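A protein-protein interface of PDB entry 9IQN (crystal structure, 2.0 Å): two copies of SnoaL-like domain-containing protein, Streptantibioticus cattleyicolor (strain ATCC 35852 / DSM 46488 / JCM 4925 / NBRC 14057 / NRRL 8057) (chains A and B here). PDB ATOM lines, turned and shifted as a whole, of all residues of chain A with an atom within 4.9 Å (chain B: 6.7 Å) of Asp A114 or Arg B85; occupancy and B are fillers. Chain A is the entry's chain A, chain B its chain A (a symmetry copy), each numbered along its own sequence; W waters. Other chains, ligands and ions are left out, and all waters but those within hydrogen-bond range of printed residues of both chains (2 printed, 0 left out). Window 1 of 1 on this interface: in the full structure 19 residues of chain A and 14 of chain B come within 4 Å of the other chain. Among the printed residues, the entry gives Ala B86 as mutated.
The backbone NH (N) of Ile A32 sits at hydrogen-bond distance from the backbone carbonyl oxygen (O) of Lys A113 (2.7 Å). The backbone NH (N) of Lys B70 is in hydrogen-bond range of the backbone carbonyl oxygen (O) of Thr B87, 2.7 Å away. The backbone NH (N) of Val A100 lies within hydrogen-bond range of the backbone carbonyl oxygen (O) of Tyr A116 (2.9 Å). The backbone carbonyl oxygen (O) of Arg B85 sits at hydrogen-bond distance from the backbone NH (N) of Glu B72 (2.9 Å). The backbone carbonyl oxygen (O) of Asp A114 lies within hydrogen-bond range of the backbone NH (N) of Leu A102. NH2 of Arg B85 lies within hydrogen-bond range of OG1 of Thr B87 (3.2 Å).
Printed residues of chain A that touch a printed residue of chain B: Ile A32, Leu A102, Leu A112, Asp A114, Val A115 and Tyr A116. Hydrophobic or aromatic side chains of chain A within 4 Å of the printed part of chain B: Ile A32, Leu A102, Leu A112 and Tyr A116.
Water W1 lies within hydrogen-bond range of OH of Tyr A116 and NH1 of Arg B85. Water W2 bridges O of Val A115 (3.0 Å) and NH1 of Arg B98 (3.4 Å).
Asp A114 touches just these residues of chain B: Arg B85 (2.8 Å) and Arg B98 (2.9 Å). Arg B85 touches four residues of chain A. Of the printed residues of chain A, Glu B72 touches Leu A112 (3.9 Å). Printed residues of chain B within 4 Å of Val A115: Arg B98 (3.5 Å). The nearest residue of chain A that does not touch Arg B85 is Ile A32 (4.03 Å).
Positions printed for both chains: 100 and 101.
Among the printed residues, merely in contact across the chains: Ile A32 with Thr B87 (3.9 Å), Ile A32 with Val B95 (3.8 Å), Ile A32 with Arg B98 (3.8 Å), Leu A102 with Arg B85 (3.8 Å), Leu A112 with Glu B72 (3.9 Å), Leu A112 with Arg B85 (3.9 Å), Val A115 with Arg B98 (3.5 Å) and Tyr A116 with Arg B98 (3.9 Å).
The guanidinium group (NH1) of Arg B85 sits at hydrogen-bond distance from the side-chain hydroxyl (OH) of Tyr A116, at 2.5 Å. The side-chain carboxylate of Asp A114 lies within salt-bridge range of the guanidinium group of Arg B98 (2.9 Å). The guanidinium group (NH2) of Arg B85 is in salt-bridge range of the side-chain carboxylate (OD2) of Asp A114 (2.8 Å).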
ATOM      1  N   ILE A  32      -2.282 -31.857 -30.445  1.00  0.00           N
ATOM      2  CA  ILE A  32      -1.303 -32.875 -30.080  1.00  0.00           C
ATOM      3  C   ILE A  32      -1.944 -33.841 -29.098  1.00  0.00           C
ATOM      4  O   ILE A  32      -2.453 -33.424 -28.049  1.00  0.00           O
ATOM      5  CB  ILE A  32      -0.041 -32.237 -29.484  1.00  0.00           C
ATOM      6  CG1 ILE A  32       0.579 -31.283 -30.520  1.00  0.00           C
ATOM      7  CG2 ILE A  32       0.954 -33.310 -29.043  1.00  0.00           C
ATOM      8  CD1 ILE A  32       1.826 -30.625 -30.044  1.00  0.00           C
ATOM      9  N   VAL A 100      -4.228 -31.575 -17.678  1.00  0.00           N
ATOM     10  CA  VAL A 100      -4.549 -30.206 -18.035  1.00  0.00           C
ATOM     11  C   VAL A 100      -4.457 -30.129 -19.543  1.00  0.00           C
ATOM     12  O   VAL A 100      -3.449 -30.560 -20.114  1.00  0.00           O
ATOM     13  CB  VAL A 100      -3.582 -29.225 -17.343  1.00  0.00           C
ATOM     14  CG1 VAL A 100      -3.849 -27.793 -17.749  1.00  0.00           C
ATOM     15  CG2 VAL A 100      -3.701 -29.395 -15.816  1.00  0.00           C
ATOM     16  N   ASP A 101      -5.529 -29.661 -20.190  1.00  0.00           N
ATOM     17  CA  ASP A 101      -5.520 -29.375 -21.619  1.00  0.00           C
ATOM     18  C   ASP A 101      -5.046 -27.937 -21.801  1.00  0.00           C
ATOM     19  O   ASP A 101      -5.652 -27.012 -21.252  1.00  0.00           O
ATOM     20  CB  ASP A 101      -6.914 -29.530 -22.238  1.00  0.00           C
ATOM     21  CG  ASP A 101      -7.232 -30.974 -22.634  1.00  0.00           C
ATOM     22  OD1 ASP A 101      -8.359 -31.234 -23.137  1.00  0.00           O
ATOM     23  OD2 ASP A 101      -6.373 -31.878 -22.407  1.00  0.00           O
ATOM     24  N   LEU A 102      -3.961 -27.757 -22.551  1.00  0.00           N
ATOM     25  CA  LEU A 102      -3.460 -26.438 -22.915  1.00  0.00           C
ATOM     26  C   LEU A 102      -4.090 -25.986 -24.227  1.00  0.00           C
ATOM     27  O   LEU A 102      -4.092 -26.728 -25.210  1.00  0.00           O
ATOM     28  CB  LEU A 102      -1.941 -26.464 -23.063  1.00  0.00           C
ATOM     29  CG  LEU A 102      -1.315 -25.191 -23.669  1.00  0.00           C
ATOM     30  CD1 LEU A 102      -1.411 -24.000 -22.734  1.00  0.00           C
ATOM     31  CD2 LEU A 102       0.137 -25.429 -24.082  1.00  0.00           C
ATOM     32  N   LEU A 112      -2.920 -24.230 -30.946  1.00  0.00           N
ATOM     33  CA  LEU A 112      -2.300 -25.398 -30.328  1.00  0.00           C
ATOM     34  C   LEU A 112      -3.234 -25.903 -29.249  1.00  0.00           C
ATOM     35  O   LEU A 112      -3.623 -25.130 -28.365  1.00  0.00           O
ATOM     36  CB  LEU A 112      -0.934 -25.067 -29.717  1.00  0.00           C
ATOM     37  CG  LEU A 112      -0.269 -26.296 -29.093  1.00  0.00           C
ATOM     38  CD1 LEU A 112       0.421 -27.127 -30.152  1.00  0.00           C
ATOM     39  CD2 LEU A 112       0.713 -25.857 -28.018  1.00  0.00           C
ATOM     40  N   LYS A 113      -3.608 -27.173 -29.345  1.00  0.00           N
ATOM     41  CA  LYS A 113      -4.217 -27.902 -28.233  1.00  0.00           C
ATOM     42  C   LYS A 113      -3.264 -29.024 -27.842  1.00  0.00           C
ATOM     43  O   LYS A 113      -2.923 -29.864 -28.677  1.00  0.00           O
ATOM     44  CB  LYS A 113      -5.586 -28.485 -28.624  1.00  0.00           C
ATOM     45  CG  LYS A 113      -6.227 -29.346 -27.490  1.00  0.00           C
ATOM     46  CD  LYS A 113      -7.561 -29.909 -27.947  1.00  0.00           C
ATOM     47  CE  LYS A 113      -8.329 -30.563 -26.817  1.00  0.00           C
ATOM     48  NZ  LYS A 113      -7.761 -31.848 -26.380  1.00  0.00           N
ATOM     49  N   ASP A 114      -2.816 -29.041 -26.594  1.00  0.00           N
ATOM     50  CA  ASP A 114      -1.949 -30.121 -26.152  1.00  0.00           C
ATOM     51  C   ASP A 114      -2.415 -30.573 -24.781  1.00  0.00           C
ATOM     52  O   ASP A 114      -3.217 -29.924 -24.125  1.00  0.00           O
ATOM     53  CB  ASP A 114      -0.473 -29.704 -26.116  1.00  0.00           C
ATOM     54  CG  ASP A 114       0.502 -30.905 -26.029  1.00  0.00           C
ATOM     55  OD1 ASP A 114       0.091 -32.090 -26.088  1.00  0.00           O
ATOM     56  OD2 ASP A 114       1.716 -30.653 -25.928  1.00  0.00           O
ATOM     57  N   VAL A 115      -1.931 -31.708 -24.343  1.00  0.00           N
ATOM     58  CA  VAL A 115      -2.337 -32.220 -23.043  1.00  0.00           C
ATOM     59  C   VAL A 115      -1.108 -32.594 -22.248  1.00  0.00           C
ATOM     60  O   VAL A 115      -0.114 -33.069 -22.805  1.00  0.00           O
ATOM     61  CB  VAL A 115      -3.260 -33.440 -23.157  1.00  0.00           C
ATOM     62  CG1 VAL A 115      -2.408 -34.672 -23.369  1.00  0.00           C
ATOM     63  CG2 VAL A 115      -4.053 -33.562 -21.858  1.00  0.00           C
ATOM     64  N   TYR A 116      -1.176 -32.353 -20.952  1.00  0.00           N
ATOM     65  CA  TYR A 116      -0.240 -32.906 -20.004  1.00  0.00           C
ATOM     66  C   TYR A 116      -1.072 -33.798 -19.095  1.00  0.00           C
ATOM     67  O   TYR A 116      -2.158 -33.398 -18.653  1.00  0.00           O
ATOM     68  CB  TYR A 116       0.495 -31.802 -19.258  1.00  0.00           C
ATOM     69  CG  TYR A 116       1.197 -30.735 -20.134  1.00  0.00           C
ATOM     70  CD1 TYR A 116       0.473 -29.720 -20.750  1.00  0.00           C
ATOM     71  CD2 TYR A 116       2.589 -30.733 -20.312  1.00  0.00           C
ATOM     72  CE1 TYR A 116       1.109 -28.735 -21.520  1.00  0.00           C
ATOM     73  CE2 TYR A 116       3.237 -29.746 -21.082  1.00  0.00           C
ATOM     74  CZ  TYR A 116       2.474 -28.748 -21.680  1.00  0.00           C
ATOM     75  OH  TYR A 116       3.068 -27.746 -22.436  1.00  0.00           O
ATOM     76  N   LYS B  70       8.748 -25.287 -33.566  1.00  0.00           N
ATOM     77  CA  LYS B  70       7.636 -24.381 -33.786  1.00  0.00           C
ATOM     78  C   LYS B  70       7.417 -23.616 -32.490  1.00  0.00           C
ATOM     79  O   LYS B  70       7.229 -24.231 -31.436  1.00  0.00           O
ATOM     80  CB  LYS B  70       6.393 -25.158 -34.194  1.00  0.00           C
ATOM     81  CG  LYS B  70       5.110 -24.355 -34.199  1.00  0.00           C
ATOM     82  CD  LYS B  70       4.015 -25.122 -34.940  1.00  0.00           C
ATOM     83  CE  LYS B  70       4.477 -25.550 -36.349  1.00  0.00           C
ATOM     84  NZ  LYS B  70       3.348 -25.572 -37.347  1.00  0.00           N
ATOM     85  N   PHE B  71       7.481 -22.286 -32.547  1.00  0.00           N
ATOM     86  CA  PHE B  71       7.352 -21.446 -31.361  1.00  0.00           C
ATOM     87  C   PHE B  71       6.019 -20.722 -31.397  1.00  0.00           C
ATOM     88  O   PHE B  71       5.685 -20.114 -32.414  1.00  0.00           O
ATOM     89  CB  PHE B  71       8.494 -20.430 -31.273  1.00  0.00           C
ATOM     90  CG  PHE B  71       9.846 -21.070 -31.156  1.00  0.00           C
ATOM     91  CD1 PHE B  71      10.349 -21.420 -29.913  1.00  0.00           C
ATOM     92  CD2 PHE B  71      10.601 -21.344 -32.282  1.00  0.00           C
ATOM     93  CE1 PHE B  71      11.595 -22.013 -29.794  1.00  0.00           C
ATOM     94  CE2 PHE B  71      11.837 -21.931 -32.174  1.00  0.00           C
ATOM     95  CZ  PHE B  71      12.330 -22.275 -30.921  1.00  0.00           C
ATOM     96  N   GLU B  72       5.283 -20.766 -30.287  1.00  0.00           N
ATOM     97  CA  GLU B  72       4.037 -20.031 -30.163  1.00  0.00           C
ATOM     98  C   GLU B  72       4.309 -18.581 -29.749  1.00  0.00           C
ATOM     99  O   GLU B  72       5.404 -18.223 -29.306  1.00  0.00           O
ATOM    100  CB  GLU B  72       3.110 -20.693 -29.151  1.00  0.00           C
ATOM    101  CG  GLU B  72       2.897 -22.183 -29.384  1.00  0.00           C
ATOM    102  CD  GLU B  72       2.235 -22.453 -30.714  1.00  0.00           C
ATOM    103  OE1 GLU B  72       1.577 -21.535 -31.250  1.00  0.00           O
ATOM    104  OE2 GLU B  72       2.376 -23.571 -31.236  1.00  0.00           O
ATOM    105  N   SER B  73       3.295 -17.738 -29.900  1.00  0.00           N
ATOM    106  CA  SER B  73       3.410 -16.353 -29.463  1.00  0.00           C
ATOM    107  C   SER B  73       3.558 -16.304 -27.948  1.00  0.00           C
ATOM    108  O   SER B  73       2.961 -17.118 -27.242  1.00  0.00           O
ATOM    109  CB  SER B  73       2.190 -15.571 -29.880  1.00  0.00           C
ATOM    110  OG  SER B  73       2.405 -14.995 -31.148  1.00  0.00           O
ATOM    111  N   PRO B  74       4.355 -15.386 -27.416  1.00  0.00           N
ATOM    112  CA  PRO B  74       4.612 -15.406 -25.970  1.00  0.00           C
ATOM    113  C   PRO B  74       3.342 -15.120 -25.185  1.00  0.00           C
ATOM    114  O   PRO B  74       2.520 -14.290 -25.577  1.00  0.00           O
ATOM    115  CB  PRO B  74       5.658 -14.300 -25.777  1.00  0.00           C
ATOM    116  CG  PRO B  74       5.515 -13.446 -26.980  1.00  0.00           C
ATOM    117  CD  PRO B  74       5.160 -14.365 -28.095  1.00  0.00           C
ATOM    118  N   ILE B  75       3.181 -15.824 -24.072  1.00  0.00           N
ATOM    119  CA  ILE B  75       2.116 -15.545 -23.115  1.00  0.00           C
ATOM    120  C   ILE B  75       2.698 -14.677 -22.010  1.00  0.00           C
ATOM    121  O   ILE B  75       3.629 -15.103 -21.321  1.00  0.00           O
ATOM    122  CB  ILE B  75       1.530 -16.841 -22.535  1.00  0.00           C
ATOM    123  CG1 ILE B  75       1.066 -17.770 -23.666  1.00  0.00           C
ATOM    124  CG2 ILE B  75       0.436 -16.501 -21.519  1.00  0.00           C
ATOM    125  CD1 ILE B  75      -0.005 -17.150 -24.591  1.00  0.00           C
ATOM    126  N   LEU B  83       6.182 -16.315 -21.360  1.00  0.00           N
ATOM    127  CA  LEU B  83       6.421 -17.727 -21.620  1.00  0.00           C
ATOM    128  C   LEU B  83       6.115 -18.044 -23.079  1.00  0.00           C
ATOM    129  O   LEU B  83       5.063 -17.667 -23.584  1.00  0.00           O
ATOM    130  CB  LEU B  83       5.581 -18.626 -20.709  1.00  0.00           C
ATOM    131  CG  LEU B  83       5.720 -18.509 -19.193  1.00  0.00           C
ATOM    132  CD1 LEU B  83       4.828 -19.546 -18.492  1.00  0.00           C
ATOM    133  CD2 LEU B  83       7.170 -18.681 -18.809  1.00  0.00           C
ATOM    134  N   VAL B  84       7.015 -18.770 -23.738  1.00  0.00           N
ATOM    135  CA  VAL B  84       6.876 -19.147 -25.140  1.00  0.00           C
ATOM    136  C   VAL B  84       6.883 -20.666 -25.199  1.00  0.00           C
ATOM    137  O   VAL B  84       7.881 -21.301 -24.827  1.00  0.00           O
ATOM    138  CB  VAL B  84       8.000 -18.553 -26.001  1.00  0.00           C
ATOM    139  CG1 VAL B  84       7.959 -19.140 -27.419  1.00  0.00           C
ATOM    140  CG2 VAL B  84       7.889 -17.035 -26.051  1.00  0.00           C
ATOM    141  N   ARG B  85       5.777 -21.250 -25.641  1.00  0.00           N
ATOM    142  CA  ARG B  85       5.715 -22.692 -25.819  1.00  0.00           C
ATOM    143  C   ARG B  85       6.485 -23.067 -27.084  1.00  0.00           C
ATOM    144  O   ARG B  85       6.333 -22.426 -28.122  1.00  0.00           O
ATOM    145  CB  ARG B  85       4.257 -23.160 -25.896  1.00  0.00           C
ATOM    146  CG  ARG B  85       4.073 -24.550 -26.460  1.00  0.00           C
ATOM    147  CD  ARG B  85       4.742 -25.640 -25.579  1.00  0.00           C
ATOM    148  NE  ARG B  85       4.655 -26.922 -26.261  1.00  0.00           N
ATOM    149  CZ  ARG B  85       3.756 -27.859 -26.006  1.00  0.00           C
ATOM    150  NH1 ARG B  85       3.005 -27.823 -24.911  1.00  0.00           N
ATOM    151  NH2 ARG B  85       3.578 -28.839 -26.889  1.00  0.00           N
ATOM    152  N   ALA B  86       7.349 -24.076 -26.987  1.00  0.00           N
ATOM    153  CA  ALA B  86       8.048 -24.627 -28.138  1.00  0.00           C
ATOM    154  C   ALA B  86       7.702 -26.107 -28.271  1.00  0.00           C
ATOM    155  O   ALA B  86       7.494 -26.799 -27.266  1.00  0.00           O
ATOM    156  CB  ALA B  86       9.568 -24.440 -28.035  1.00  0.00           C
ATOM    157  N   THR B  87       7.557 -26.545 -29.520  1.00  0.00           N
ATOM    158  CA  THR B  87       7.334 -27.929 -29.912  1.00  0.00           C
ATOM    159  C   THR B  87       8.275 -28.260 -31.063  1.00  0.00           C
ATOM    160  O   THR B  87       8.292 -27.544 -32.070  1.00  0.00           O
ATOM    161  CB  THR B  87       5.892 -28.150 -30.373  1.00  0.00           C
ATOM    162  OG1 THR B  87       4.987 -27.569 -29.433  1.00  0.00           O
ATOM    163  CG2 THR B  87       5.604 -29.626 -30.502  1.00  0.00           C
ATOM    164  N   GLU B  89       8.973 -31.023 -33.897  1.00  0.00           N
ATOM    165  CA  GLU B  89       8.153 -32.021 -34.579  1.00  0.00           C
ATOM    166  C   GLU B  89       8.862 -32.573 -35.805  1.00  0.00           C
ATOM    167  O   GLU B  89       9.543 -31.830 -36.510  1.00  0.00           O
ATOM    168  CB  GLU B  89       6.811 -31.404 -35.017  1.00  0.00           C
ATOM    169  CG  GLU B  89       5.999 -30.910 -33.830  1.00  0.00           C
ATOM    170  CD  GLU B  89       4.875 -29.979 -34.212  1.00  0.00           C
ATOM    171  OE1 GLU B  89       4.708 -29.693 -35.415  1.00  0.00           O
ATOM    172  OE2 GLU B  89       4.164 -29.530 -33.291  1.00  0.00           O
ATOM    173  N   VAL B  95       5.886 -35.432 -32.312  1.00  0.00           N
ATOM    174  CA  VAL B  95       6.557 -34.555 -31.359  1.00  0.00           C
ATOM    175  C   VAL B  95       7.777 -35.291 -30.830  1.00  0.00           C
ATOM    176  O   VAL B  95       7.670 -36.409 -30.309  1.00  0.00           O
ATOM    177  CB  VAL B  95       5.616 -34.140 -30.221  1.00  0.00           C
ATOM    178  CG1 VAL B  95       6.312 -33.140 -29.290  1.00  0.00           C
ATOM    179  CG2 VAL B  95       4.359 -33.541 -30.789  1.00  0.00           C
ATOM    180  N   ASN B  97      10.263 -33.214 -29.056  1.00  0.00           N
ATOM    181  CA  ASN B  97      10.628 -32.486 -27.857  1.00  0.00           C
ATOM    182  C   ASN B  97       9.634 -31.349 -27.675  1.00  0.00           C
ATOM    183  O   ASN B  97       8.994 -30.900 -28.632  1.00  0.00           O
ATOM    184  CB  ASN B  97      12.060 -31.937 -27.918  1.00  0.00           C
ATOM    185  CG  ASN B  97      12.667 -31.759 -26.535  1.00  0.00           C
ATOM    186  OD1 ASN B  97      12.035 -32.060 -25.542  1.00  0.00           O
ATOM    187  ND2 ASN B  97      13.909 -31.327 -26.478  1.00  0.00           N
ATOM    188  N   ARG B  98       9.508 -30.900 -26.434  1.00  0.00           N
ATOM    189  CA  ARG B  98       8.659 -29.764 -26.125  1.00  0.00           C
ATOM    190  C   ARG B  98       9.271 -29.040 -24.936  1.00  0.00           C
ATOM    191  O   ARG B  98      10.012 -29.621 -24.137  1.00  0.00           O
ATOM    192  CB  ARG B  98       7.217 -30.214 -25.820  1.00  0.00           C
ATOM    193  CG  ARG B  98       7.128 -31.086 -24.605  1.00  0.00           C
ATOM    194  CD  ARG B  98       5.680 -31.217 -24.126  1.00  0.00           C
ATOM    195  NE  ARG B  98       4.905 -31.894 -25.147  1.00  0.00           N
ATOM    196  CZ  ARG B  98       3.781 -32.553 -24.930  1.00  0.00           C
ATOM    197  NH1 ARG B  98       3.246 -32.626 -23.715  1.00  0.00           N
ATOM    198  NH2 ARG B  98       3.182 -33.162 -25.956  1.00  0.00           N
ATOM    199  N   GLY B  99       8.953 -27.763 -24.832  1.00  0.00           N
ATOM    200  CA  GLY B  99       9.465 -26.999 -23.727  1.00  0.00           C
ATOM    201  C   GLY B  99       8.863 -25.621 -23.709  1.00  0.00           C
ATOM    202  O   GLY B  99       7.969 -25.303 -24.488  1.00  0.00           O
ATOM    203  N   VAL B 100       9.391 -24.808 -22.808  1.00  0.00           N
ATOM    204  CA  VAL B 100       8.906 -23.458 -22.583  1.00  0.00           C
ATOM    205  C   VAL B 100      10.133 -22.579 -22.485  1.00  0.00           C
ATOM    206  O   VAL B 100      11.053 -22.901 -21.726  1.00  0.00           O
ATOM    207  CB  VAL B 100       8.044 -23.399 -21.306  1.00  0.00           C
ATOM    208  CG1 VAL B 100       7.579 -21.991 -21.008  1.00  0.00           C
ATOM    209  CG2 VAL B 100       6.844 -24.352 -21.466  1.00  0.00           C
ATOM    210  N   ASP B 101      10.185 -21.522 -23.302  1.00  0.00           N
ATOM    211  CA  ASP B 101      11.220 -20.501 -23.200  1.00  0.00           C
ATOM    212  C   ASP B 101      10.732 -19.446 -22.212  1.00  0.00           C
ATOM    213  O   ASP B 101       9.665 -18.858 -22.411  1.00  0.00           O
ATOM    214  CB  ASP B 101      11.500 -19.836 -24.552  1.00  0.00           C
ATOM    215  CG  ASP B 101      12.501 -20.620 -25.404  1.00  0.00           C
ATOM    216  OD1 ASP B 101      12.799 -20.184 -26.550  1.00  0.00           O
ATOM    217  OD2 ASP B 101      12.974 -21.707 -24.955  1.00  0.00           O
HETATM  218  O   HOH W   1       5.623 -27.542 -22.974  1.00  0.00           O
HETATM  219  O   HOH W   2       1.308 -35.425 -23.880  1.00  0.00           O
